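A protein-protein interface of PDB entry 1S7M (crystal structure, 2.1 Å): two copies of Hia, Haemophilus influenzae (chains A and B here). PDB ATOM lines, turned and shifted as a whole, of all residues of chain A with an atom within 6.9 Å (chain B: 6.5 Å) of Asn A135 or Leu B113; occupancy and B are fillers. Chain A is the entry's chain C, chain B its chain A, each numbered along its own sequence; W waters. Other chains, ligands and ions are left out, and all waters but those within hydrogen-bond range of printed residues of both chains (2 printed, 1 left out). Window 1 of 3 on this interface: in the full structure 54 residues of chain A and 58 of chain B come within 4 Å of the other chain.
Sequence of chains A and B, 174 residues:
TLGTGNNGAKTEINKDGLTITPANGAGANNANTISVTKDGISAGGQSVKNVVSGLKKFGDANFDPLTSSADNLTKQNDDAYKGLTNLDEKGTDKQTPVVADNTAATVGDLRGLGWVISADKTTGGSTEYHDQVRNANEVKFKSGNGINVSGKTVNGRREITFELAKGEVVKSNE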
ATOM      1  N   LEU A 110      -3.901  16.985 -16.215  1.00  0.00           N
ATOM      2  CA  LEU A 110      -2.477  17.335 -16.170  1.00  0.00           C
ATOM      3  C   LEU A 110      -2.179  18.690 -16.845  1.00  0.00           C
ATOM      4  O   LEU A 110      -1.352  19.472 -16.377  1.00  0.00           O
ATOM      5  CB  LEU A 110      -1.615  16.259 -16.861  1.00  0.00           C
ATOM      6  CG  LEU A 110      -1.591  14.810 -16.344  1.00  0.00           C
ATOM      7  CD1 LEU A 110      -0.350  14.117 -16.915  1.00  0.00           C
ATOM      8  CD2 LEU A 110      -1.544  14.759 -14.814  1.00  0.00           C
ATOM      9  N   ARG A 111      -2.858  18.942 -17.960  1.00  0.00           N
ATOM     10  CA  ARG A 111      -2.682  20.176 -18.696  1.00  0.00           C
ATOM     11  C   ARG A 111      -3.046  21.418 -17.877  1.00  0.00           C
ATOM     12  O   ARG A 111      -2.530  22.486 -18.126  1.00  0.00           O
ATOM     13  CB  ARG A 111      -3.497  20.120 -20.016  1.00  0.00           C
ATOM     14  CG  ARG A 111      -2.822  19.236 -21.076  1.00  0.00           C
ATOM     15  CD  ARG A 111      -3.631  19.085 -22.414  1.00  0.00           C
ATOM     16  NE  ARG A 111      -2.853  18.322 -23.394  1.00  0.00           N
ATOM     17  CZ  ARG A 111      -3.341  17.349 -24.160  1.00  0.00           C
ATOM     18  NH1 ARG A 111      -4.620  17.003 -24.093  1.00  0.00           N
ATOM     19  NH2 ARG A 111      -2.536  16.689 -24.983  1.00  0.00           N
ATOM     20  N   LEU A 113      -2.453  21.657 -14.620  1.00  0.00           N
ATOM     21  CA  LEU A 113      -1.636  21.687 -13.400  1.00  0.00           C
ATOM     22  C   LEU A 113      -0.653  22.857 -13.395  1.00  0.00           C
ATOM     23  O   LEU A 113      -0.028  23.129 -14.409  1.00  0.00           O
ATOM     24  CB  LEU A 113      -0.863  20.376 -13.276  1.00  0.00           C
ATOM     25  CG  LEU A 113      -1.232  19.276 -12.269  1.00  0.00           C
ATOM     26  CD1 LEU A 113      -2.668  19.338 -11.779  1.00  0.00           C
ATOM     27  CD2 LEU A 113      -0.906  17.974 -12.886  1.00  0.00           C
ATOM     28  N   GLY A 114      -0.534  23.567 -12.270  1.00  0.00           N
ATOM     29  CA  GLY A 114       0.429  24.653 -12.205  1.00  0.00           C
ATOM     30  C   GLY A 114       0.379  25.543 -10.977  1.00  0.00           C
ATOM     31  O   GLY A 114      -0.552  25.462 -10.163  1.00  0.00           O
ATOM     32  N   VAL A 133       2.666  29.016 -13.975  1.00  0.00           N
ATOM     33  CA  VAL A 133       3.822  28.220 -14.334  1.00  0.00           C
ATOM     34  C   VAL A 133       3.295  26.801 -14.400  1.00  0.00           C
ATOM     35  O   VAL A 133       3.141  26.124 -13.375  1.00  0.00           O
ATOM     36  CB  VAL A 133       4.943  28.334 -13.275  1.00  0.00           C
ATOM     37  CG1 VAL A 133       6.144  27.512 -13.710  1.00  0.00           C
ATOM     38  CG2 VAL A 133       5.328  29.811 -13.090  1.00  0.00           C
ATOM     39  N   ARG A 134       2.977  26.359 -15.611  1.00  0.00           N
ATOM     40  CA  ARG A 134       2.482  25.014 -15.792  1.00  0.00           C
ATOM     41  C   ARG A 134       3.630  24.106 -16.204  1.00  0.00           C
ATOM     42  O   ARG A 134       4.781  24.519 -16.156  1.00  0.00           O
ATOM     43  CB  ARG A 134       1.356  25.000 -16.823  1.00  0.00           C
ATOM     44  CG  ARG A 134       0.124  25.791 -16.363  1.00  0.00           C
ATOM     45  CD  ARG A 134      -1.082  25.501 -17.236  1.00  0.00           C
ATOM     46  NE  ARG A 134      -2.109  26.537 -17.133  1.00  0.00           N
ATOM     47  CZ  ARG A 134      -3.311  26.460 -17.704  1.00  0.00           C
ATOM     48  NH1 ARG A 134      -3.640  25.383 -18.427  1.00  0.00           N
ATOM     49  NH2 ARG A 134      -4.197  27.454 -17.545  1.00  0.00           N
ATOM     50  N   ASN A 135       3.330  22.871 -16.594  1.00  0.00           N
ATOM     51  CA  ASN A 135       4.364  21.930 -16.987  1.00  0.00           C
ATOM     52  C   ASN A 135       5.147  22.514 -18.155  1.00  0.00           C
ATOM     53  O   ASN A 135       4.565  23.072 -19.072  1.00  0.00           O
ATOM     54  CB  ASN A 135       3.758  20.588 -17.402  1.00  0.00           C
ATOM     55  CG  ASN A 135       4.809  19.607 -17.859  1.00  0.00           C
ATOM     56  OD1 ASN A 135       5.627  19.155 -17.056  1.00  0.00           O
ATOM     57  ND2 ASN A 135       4.824  19.287 -19.160  1.00  0.00           N
ATOM     58  N   ALA A 136       6.467  22.391 -18.094  1.00  0.00           N
ATOM     59  CA  ALA A 136       7.359  22.873 -19.134  1.00  0.00           C
ATOM     60  C   ALA A 136       7.409  24.389 -19.329  1.00  0.00           C
ATOM     61  O   ALA A 136       7.858  24.864 -20.365  1.00  0.00           O
ATOM     62  CB  ALA A 136       7.074  22.175 -20.477  1.00  0.00           C
ATOM     63  N   ASN A 137       6.920  25.147 -18.356  1.00  0.00           N
ATOM     64  CA  ASN A 137       7.079  26.575 -18.415  1.00  0.00           C
ATOM     65  C   ASN A 137       8.444  26.831 -17.741  1.00  0.00           C
ATOM     66  O   ASN A 137       8.983  25.977 -16.995  1.00  0.00           O
ATOM     67  CB  ASN A 137       5.951  27.302 -17.687  1.00  0.00           C
ATOM     68  CG  ASN A 137       4.775  27.591 -18.595  1.00  0.00           C
ATOM     69  OD1 ASN A 137       4.948  27.989 -19.763  1.00  0.00           O
ATOM     70  ND2 ASN A 137       3.585  27.403 -18.081  1.00  0.00           N
ATOM     71  N   GLU A 138       9.026  27.978 -18.035  1.00  0.00           N
ATOM     72  CA  GLU A 138      10.332  28.328 -17.501  1.00  0.00           C
ATOM     73  C   GLU A 138      10.304  29.638 -16.722  1.00  0.00           C
ATOM     74  O   GLU A 138       9.662  30.604 -17.141  1.00  0.00           O
ATOM     75  CB  GLU A 138      11.358  28.432 -18.648  1.00  0.00           C
ATOM     76  CG  GLU A 138      12.719  28.973 -18.203  1.00  0.00           C
ATOM     77  CD  GLU A 138      13.733  29.083 -19.352  1.00  0.00           C
ATOM     78  OE1 GLU A 138      14.769  29.744 -19.176  1.00  0.00           O
ATOM     79  OE2 GLU A 138      13.482  28.502 -20.423  1.00  0.00           O
ATOM     80  N   LYS B  57       8.021  12.339 -23.815  1.00  0.00           N
ATOM     81  CA  LYS B  57       8.870  13.244 -23.061  1.00  0.00           C
ATOM     82  C   LYS B  57       9.573  14.079 -24.108  1.00  0.00           C
ATOM     83  O   LYS B  57       9.806  13.599 -25.213  1.00  0.00           O
ATOM     84  CB  LYS B  57       9.929  12.457 -22.280  1.00  0.00           C
ATOM     85  CG  LYS B  57       9.359  11.469 -21.237  1.00  0.00           C
ATOM     86  CD  LYS B  57       8.297  12.147 -20.370  1.00  0.00           C
ATOM     87  CE  LYS B  57       8.002  11.342 -19.092  1.00  0.00           C
ATOM     88  NZ  LYS B  57       7.447  10.016 -19.399  1.00  0.00           N
ATOM     89  N   PHE B  58       9.926  15.314 -23.780  1.00  0.00           N
ATOM     90  CA  PHE B  58      10.656  16.127 -24.741  1.00  0.00           C
ATOM     91  C   PHE B  58      12.018  15.459 -24.960  1.00  0.00           C
ATOM     92  O   PHE B  58      12.680  15.021 -23.997  1.00  0.00           O
ATOM     93  CB  PHE B  58      10.866  17.557 -24.227  1.00  0.00           C
ATOM     94  CG  PHE B  58       9.635  18.427 -24.305  1.00  0.00           C
ATOM     95  CD1 PHE B  58       8.970  18.830 -23.145  1.00  0.00           C
ATOM     96  CD2 PHE B  58       9.147  18.856 -25.533  1.00  0.00           C
ATOM     97  CE1 PHE B  58       7.842  19.645 -23.204  1.00  0.00           C
ATOM     98  CE2 PHE B  58       8.013  19.679 -25.608  1.00  0.00           C
ATOM     99  CZ  PHE B  58       7.355  20.077 -24.435  1.00  0.00           C
ATOM    100  N   LYS B  75      11.437  23.278 -27.382  1.00  0.00           N
ATOM    101  CA  LYS B  75      11.560  22.493 -26.171  1.00  0.00           C
ATOM    102  C   LYS B  75      12.041  21.097 -26.527  1.00  0.00           C
ATOM    103  O   LYS B  75      12.871  20.524 -25.809  1.00  0.00           O
ATOM    104  CB  LYS B  75      10.214  22.478 -25.421  1.00  0.00           C
ATOM    105  CG  LYS B  75       9.899  23.836 -24.761  1.00  0.00           C
ATOM    106  CD  LYS B  75       8.471  23.952 -24.245  1.00  0.00           C
ATOM    107  CE  LYS B  75       8.310  25.278 -23.499  1.00  0.00           C
ATOM    108  NZ  LYS B  75       6.881  25.623 -23.243  1.00  0.00           N
ATOM    109  N   GLY B  83      13.426  15.066 -21.166  1.00  0.00           N
ATOM    110  CA  GLY B  83      12.806  14.184 -20.201  1.00  0.00           C
ATOM    111  C   GLY B  83      11.536  14.726 -19.572  1.00  0.00           C
ATOM    112  O   GLY B  83      10.782  13.966 -18.974  1.00  0.00           O
ATOM    113  N   LEU B  84      11.291  16.031 -19.681  1.00  0.00           N
ATOM    114  CA  LEU B  84      10.048  16.590 -19.134  1.00  0.00           C
ATOM    115  C   LEU B  84       8.911  16.131 -20.039  1.00  0.00           C
ATOM    116  O   LEU B  84       9.058  16.137 -21.259  1.00  0.00           O
ATOM    117  CB  LEU B  84      10.074  18.118 -19.137  1.00  0.00           C
ATOM    118  CG  LEU B  84      10.967  18.827 -18.124  1.00  0.00           C
ATOM    119  CD1 LEU B  84      10.744  20.329 -18.225  1.00  0.00           C
ATOM    120  CD2 LEU B  84      10.613  18.332 -16.720  1.00  0.00           C
ATOM    121  N   THR B  85       7.782  15.756 -19.447  1.00  0.00           N
ATOM    122  CA  THR B  85       6.610  15.307 -20.212  1.00  0.00           C
ATOM    123  C   THR B  85       6.145  16.371 -21.226  1.00  0.00           C
ATOM    124  O   THR B  85       6.098  17.562 -20.918  1.00  0.00           O
ATOM    125  CB  THR B  85       5.451  14.971 -19.255  1.00  0.00           C
ATOM    126  OG1 THR B  85       5.908  14.012 -18.287  1.00  0.00           O
ATOM    127  CG2 THR B  85       4.263  14.404 -20.008  1.00  0.00           C
ATOM    128  N   ASN B  86       5.813  15.949 -22.442  1.00  0.00           N
ATOM    129  CA  ASN B  86       5.355  16.906 -23.463  1.00  0.00           C
ATOM    130  C   ASN B  86       3.856  16.761 -23.553  1.00  0.00           C
ATOM    131  O   ASN B  86       3.362  15.749 -24.047  1.00  0.00           O
ATOM    132  CB  ASN B  86       6.004  16.603 -24.828  1.00  0.00           C
ATOM    133  CG  ASN B  86       5.412  17.459 -25.975  1.00  0.00           C
ATOM    134  OD1 ASN B  86       4.634  18.386 -25.748  1.00  0.00           O
ATOM    135  ND2 ASN B  86       5.814  17.154 -27.203  1.00  0.00           N
ATOM    136  N   LEU B  87       3.132  17.761 -23.055  1.00  0.00           N
ATOM    137  CA  LEU B  87       1.678  17.711 -23.052  1.00  0.00           C
ATOM    138  C   LEU B  87       1.023  18.318 -24.264  1.00  0.00           C
ATOM    139  O   LEU B  87      -0.194  18.267 -24.382  1.00  0.00           O
ATOM    140  CB  LEU B  87       1.116  18.435 -21.815  1.00  0.00           C
ATOM    141  CG  LEU B  87       1.541  17.863 -20.457  1.00  0.00           C
ATOM    142  CD1 LEU B  87       1.086  18.782 -19.339  1.00  0.00           C
ATOM    143  CD2 LEU B  87       0.944  16.470 -20.300  1.00  0.00           C
ATOM    144  N   ASP B  88       1.813  18.891 -25.166  1.00  0.00           N
ATOM    145  CA  ASP B  88       1.221  19.574 -26.315  1.00  0.00           C
ATOM    146  C   ASP B  88       1.590  19.053 -27.714  1.00  0.00           C
ATOM    147  O   ASP B  88       1.508  19.808 -28.685  1.00  0.00           O
ATOM    148  CB  ASP B  88       1.571  21.072 -26.248  1.00  0.00           C
ATOM    149  CG  ASP B  88       1.282  21.692 -24.880  1.00  0.00           C
ATOM    150  OD1 ASP B  88       0.166  21.493 -24.352  1.00  0.00           O
ATOM    151  OD2 ASP B  88       2.169  22.397 -24.342  1.00  0.00           O
ATOM    152  N   GLY B 108       4.014   7.262 -15.069  1.00  0.00           N
ATOM    153  CA  GLY B 108       5.152   7.673 -15.873  1.00  0.00           C
ATOM    154  C   GLY B 108       5.034   9.098 -16.388  1.00  0.00           C
ATOM    155  O   GLY B 108       6.044   9.776 -16.527  1.00  0.00           O
ATOM    156  N   ASP B 109       3.806   9.531 -16.700  1.00  0.00           N
ATOM    157  CA  ASP B 109       3.531  10.898 -17.175  1.00  0.00           C
ATOM    158  C   ASP B 109       3.851  11.840 -16.015  1.00  0.00           C
ATOM    159  O   ASP B 109       4.506  12.867 -16.198  1.00  0.00           O
ATOM    160  CB  ASP B 109       2.047  11.037 -17.590  1.00  0.00           C
ATOM    161  CG  ASP B 109       1.640  10.067 -18.723  1.00  0.00           C
ATOM    162  OD1 ASP B 109       2.532   9.590 -19.456  1.00  0.00           O
ATOM    163  OD2 ASP B 109       0.425   9.802 -18.899  1.00  0.00           O
ATOM    164  N   LEU B 110       3.391  11.479 -14.811  1.00  0.00           N
ATOM    165  CA  LEU B 110       3.656  12.280 -13.625  1.00  0.00           C
ATOM    166  C   LEU B 110       5.140  12.438 -13.340  1.00  0.00           C
ATOM    167  O   LEU B 110       5.576  13.489 -12.860  1.00  0.00           O
ATOM    168  CB  LEU B 110       3.010  11.654 -12.375  1.00  0.00           C
ATOM    169  CG  LEU B 110       1.497  11.508 -12.302  1.00  0.00           C
ATOM    170  CD1 LEU B 110       1.080  11.501 -10.820  1.00  0.00           C
ATOM    171  CD2 LEU B 110       0.809  12.657 -13.035  1.00  0.00           C
ATOM    172  N   ARG B 111       5.906  11.381 -13.601  1.00  0.00           N
ATOM    173  CA  ARG B 111       7.333  11.388 -13.342  1.00  0.00           C
ATOM    174  C   ARG B 111       8.060  12.409 -14.206  1.00  0.00           C
ATOM    175  O   ARG B 111       9.116  12.922 -13.828  1.00  0.00           O
ATOM    176  CB  ARG B 111       7.906   9.968 -13.517  1.00  0.00           C
ATOM    177  CG  ARG B 111       7.642   9.062 -12.283  1.00  0.00           C
ATOM    178  CD  ARG B 111       8.076   7.610 -12.486  1.00  0.00           C
ATOM    179  NE  ARG B 111       7.839   6.842 -11.268  1.00  0.00           N
ATOM    180  CZ  ARG B 111       7.482   5.559 -11.241  1.00  0.00           C
ATOM    181  NH1 ARG B 111       7.332   4.877 -12.366  1.00  0.00           N
ATOM    182  NH2 ARG B 111       7.209   4.970 -10.083  1.00  0.00           N
ATOM    183  N   GLY B 112       7.477  12.739 -15.353  1.00  0.00           N
ATOM    184  CA  GLY B 112       8.101  13.738 -16.189  1.00  0.00           C
ATOM    185  C   GLY B 112       7.581  15.157 -15.973  1.00  0.00           C
ATOM    186  O   GLY B 112       8.030  16.073 -16.647  1.00  0.00           O
ATOM    187  N   LEU B 113       6.652  15.374 -15.041  1.00  0.00           N
ATOM    188  CA  LEU B 113       6.139  16.739 -14.865  1.00  0.00           C
ATOM    189  C   LEU B 113       7.147  17.682 -14.229  1.00  0.00           C
ATOM    190  O   LEU B 113       7.888  17.295 -13.338  1.00  0.00           O
ATOM    191  CB  LEU B 113       4.849  16.729 -14.029  1.00  0.00           C
ATOM    192  CG  LEU B 113       3.445  16.649 -14.644  1.00  0.00           C
ATOM    193  CD1 LEU B 113       3.470  16.279 -16.115  1.00  0.00           C
ATOM    194  CD2 LEU B 113       2.590  15.679 -13.823  1.00  0.00           C
ATOM    195  N   GLY B 114       7.182  18.927 -14.695  1.00  0.00           N
ATOM    196  CA  GLY B 114       8.094  19.875 -14.097  1.00  0.00           C
ATOM    197  C   GLY B 114       8.260  21.182 -14.833  1.00  0.00           C
ATOM    198  O   GLY B 114       7.788  21.351 -15.970  1.00  0.00           O
ATOM    199  N   TRP B 115       8.894  22.134 -14.173  1.00  0.00           N
ATOM    200  CA  TRP B 115       9.151  23.400 -14.813  1.00  0.00           C
ATOM    201  C   TRP B 115      10.643  23.592 -14.853  1.00  0.00           C
ATOM    202  O   TRP B 115      11.404  22.820 -14.240  1.00  0.00           O
ATOM    203  CB  TRP B 115       8.464  24.579 -14.108  1.00  0.00           C
ATOM    204  CG  TRP B 115       8.644  24.656 -12.617  1.00  0.00           C
ATOM    205  CD1 TRP B 115       8.027  23.882 -11.675  1.00  0.00           C
ATOM    206  CD2 TRP B 115       9.469  25.591 -11.901  1.00  0.00           C
ATOM    207  NE1 TRP B 115       8.418  24.282 -10.408  1.00  0.00           N
ATOM    208  CE2 TRP B 115       9.297  25.325 -10.517  1.00  0.00           C
ATOM    209  CE3 TRP B 115      10.331  26.634 -12.297  1.00  0.00           C
ATOM    210  CZ2 TRP B 115       9.954  26.063  -9.524  1.00  0.00           C
ATOM    211  CZ3 TRP B 115      10.986  27.370 -11.317  1.00  0.00           C
ATOM    212  CH2 TRP B 115      10.793  27.082  -9.936  1.00  0.00           C
ATOM    213  N   VAL B 133      12.683  21.402 -12.177  1.00  0.00           N
ATOM    214  CA  VAL B 133      12.058  21.319 -10.868  1.00  0.00           C
ATOM    215  C   VAL B 133      10.858  20.381 -11.029  1.00  0.00           C
ATOM    216  O   VAL B 133       9.763  20.794 -11.475  1.00  0.00           O
ATOM    217  CB  VAL B 133      11.551  22.684 -10.376  1.00  0.00           C
ATOM    218  CG1 VAL B 133      10.956  22.561  -8.907  1.00  0.00           C
ATOM    219  CG2 VAL B 133      12.675  23.674 -10.381  1.00  0.00           C
ATOM    220  N   ARG B 134      11.061  19.106 -10.728  1.00  0.00           N
ATOM    221  CA  ARG B 134       9.951  18.185 -10.830  1.00  0.00           C
ATOM    222  C   ARG B 134       9.361  18.000  -9.441  1.00  0.00           C
ATOM    223  O   ARG B 134       9.726  18.710  -8.498  1.00  0.00           O
ATOM    224  CB  ARG B 134      10.406  16.858 -11.418  1.00  0.00           C
ATOM    225  CG  ARG B 134      11.108  17.010 -12.743  1.00  0.00           C
ATOM    226  CD  ARG B 134      11.272  15.666 -13.406  1.00  0.00           C
ATOM    227  NE  ARG B 134      12.165  15.739 -14.558  1.00  0.00           N
ATOM    228  CZ  ARG B 134      12.401  14.719 -15.380  1.00  0.00           C
ATOM    229  NH1 ARG B 134      11.810  13.554 -15.177  1.00  0.00           N
ATOM    230  NH2 ARG B 134      13.225  14.864 -16.397  1.00  0.00           N
ATOM    231  N   ASN B 135       8.457  17.047  -9.321  1.00  0.00           N
ATOM    232  CA  ASN B 135       7.824  16.780  -8.048  1.00  0.00           C
ATOM    233  C   ASN B 135       8.907  16.456  -7.005  1.00  0.00           C
ATOM    234  O   ASN B 135       9.875  15.774  -7.314  1.00  0.00           O
ATOM    235  CB  ASN B 135       6.866  15.603  -8.217  1.00  0.00           C
ATOM    236  CG  ASN B 135       6.219  15.204  -6.939  1.00  0.00           C
ATOM    237  OD1 ASN B 135       5.469  15.976  -6.335  1.00  0.00           O
ATOM    238  ND2 ASN B 135       6.503  13.989  -6.500  1.00  0.00           N
HETATM  239  O   HOH W   1       4.024  20.195 -22.091  1.00  0.00           O
HETATM  240  O   HOH W   2       4.896  24.290 -21.743  1.00  0.00           O
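Among the printed residues, merely in contact across the chains: Asn A137 with Trp B115, Asn A135 with Leu B113, Leu A110 with Leu B110, Val A133 with Trp B115, Asn A135 with Leu B87, Ala A136 with Phe B58, Leu A110 with Leu B87, Asn A135 with Gly B112 and Leu A110 with Asp B109.
Printed residues of chain B within 4 Å of Val A133: Trp B115 (3.8 Å). Asn A135 touches just these residues of chain B: Thr B85, Leu B87, Gly B112, Leu B113 and Gly B114. Of the printed residues of chain A, Lys B75 touches Ala A136. Printed residues of chain A within 4 Å of Leu B87: Leu A110 (3.9 Å), Arg A111 (2.8 Å) and Asn A135 (3.8 Å). Leu B113 touches just one residue of chain A: Asn A135 (3.3 Å). Of the printed residues of chain A, Trp B115 touches Val A133 and Asn A137.
The backbone carbonyl oxygen (O) of Leu B84 sits at hydrogen-bond distance from the backbone NH (N) of Phe B58. OG1 of Thr B85 lies within hydrogen-bond range of O of Asp B109, 2.8 Å away. The backbone carbonyl oxygen (O) of Gly B112 is in hydrogen-bond range of the backbone NH (N) of Thr B85 (2.8 Å). The backbone NH (N) of Val B133 sits at hydrogen-bond distance from the backbone carbonyl oxygen (O) of Trp B115, at 2.8 Å. O of Arg A111 is in hydrogen-bond range of NH1 of Arg A134. The backbone NH (N) of Arg A134 sits close to the side-chain amide nitrogen (ND2) of Asn A137 (2.7 Å).
Water W1 bridges the backbone NH of Leu B87 and the side-chain amide nitrogen of Asn A135. Water W2 lies within hydrogen-bond range of the side-chain amino group of Lys B75 (2.8 Å), the backbone carbonyl oxygen of Asn A135 (3.0 Å) and the backbone carbonyl oxygen of Ala A136 (3.3 Å).
The side-chain amino group of Lys B75 sits at hydrogen-bond distance from the backbone carbonyl oxygen of Ala A136 (3.1 Å). The backbone carbonyl oxygen (O) of Thr B85 lies within hydrogen-bond range of the side-chain amide nitrogen (ND2) of Asn A135 (2.8 Å). The guanidinium group (NE) of Arg A111 lies within hydrogen-bond range of the backbone carbonyl oxygen (O) of Leu B87. The side-chain amide oxygen of Asn A135 is in hydrogen-bond range of the backbone NH of Gly B114 (2.8 Å). The backbone carbonyl oxygen (O) of Gly B114 is in hydrogen-bond range of the backbone NH (N) of Ala A136 (2.7 Å).
Leu B110 touches its own counterpart, Leu A110. Asn A135 touches Leu B113, but with the chains exchanged Leu A113 does not touch Asn B135 (9.4 Å). Asn A135 touches Gly B114, but with the chains exchanged Gly A114 does not touch Asn B135 (11.4 Å). Of the 14 pairs that touch across the chains among the printed residues, 1 has its exchanged pair printed and touching as well.
Of the 20 printed residues of chain B, 10 touch a printed residue of chain A. Hydrophobic or aromatic side chains of chain B within 4 Å of the printed part of chain A: Phe B58, Leu B87, Leu B110, Leu B113 and Trp B115. Hydrophobic or aromatic side chains of chain A within 4 Å of the printed part of chain B: Leu A110, Val A133 and Ala A136. Among the printed residues, 14 pairs touch across the chains. Among the printed residues, no Asp or Glu carboxylate lies within 4 Å of a Lys or Arg side-chain nitrogen of the other chain.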
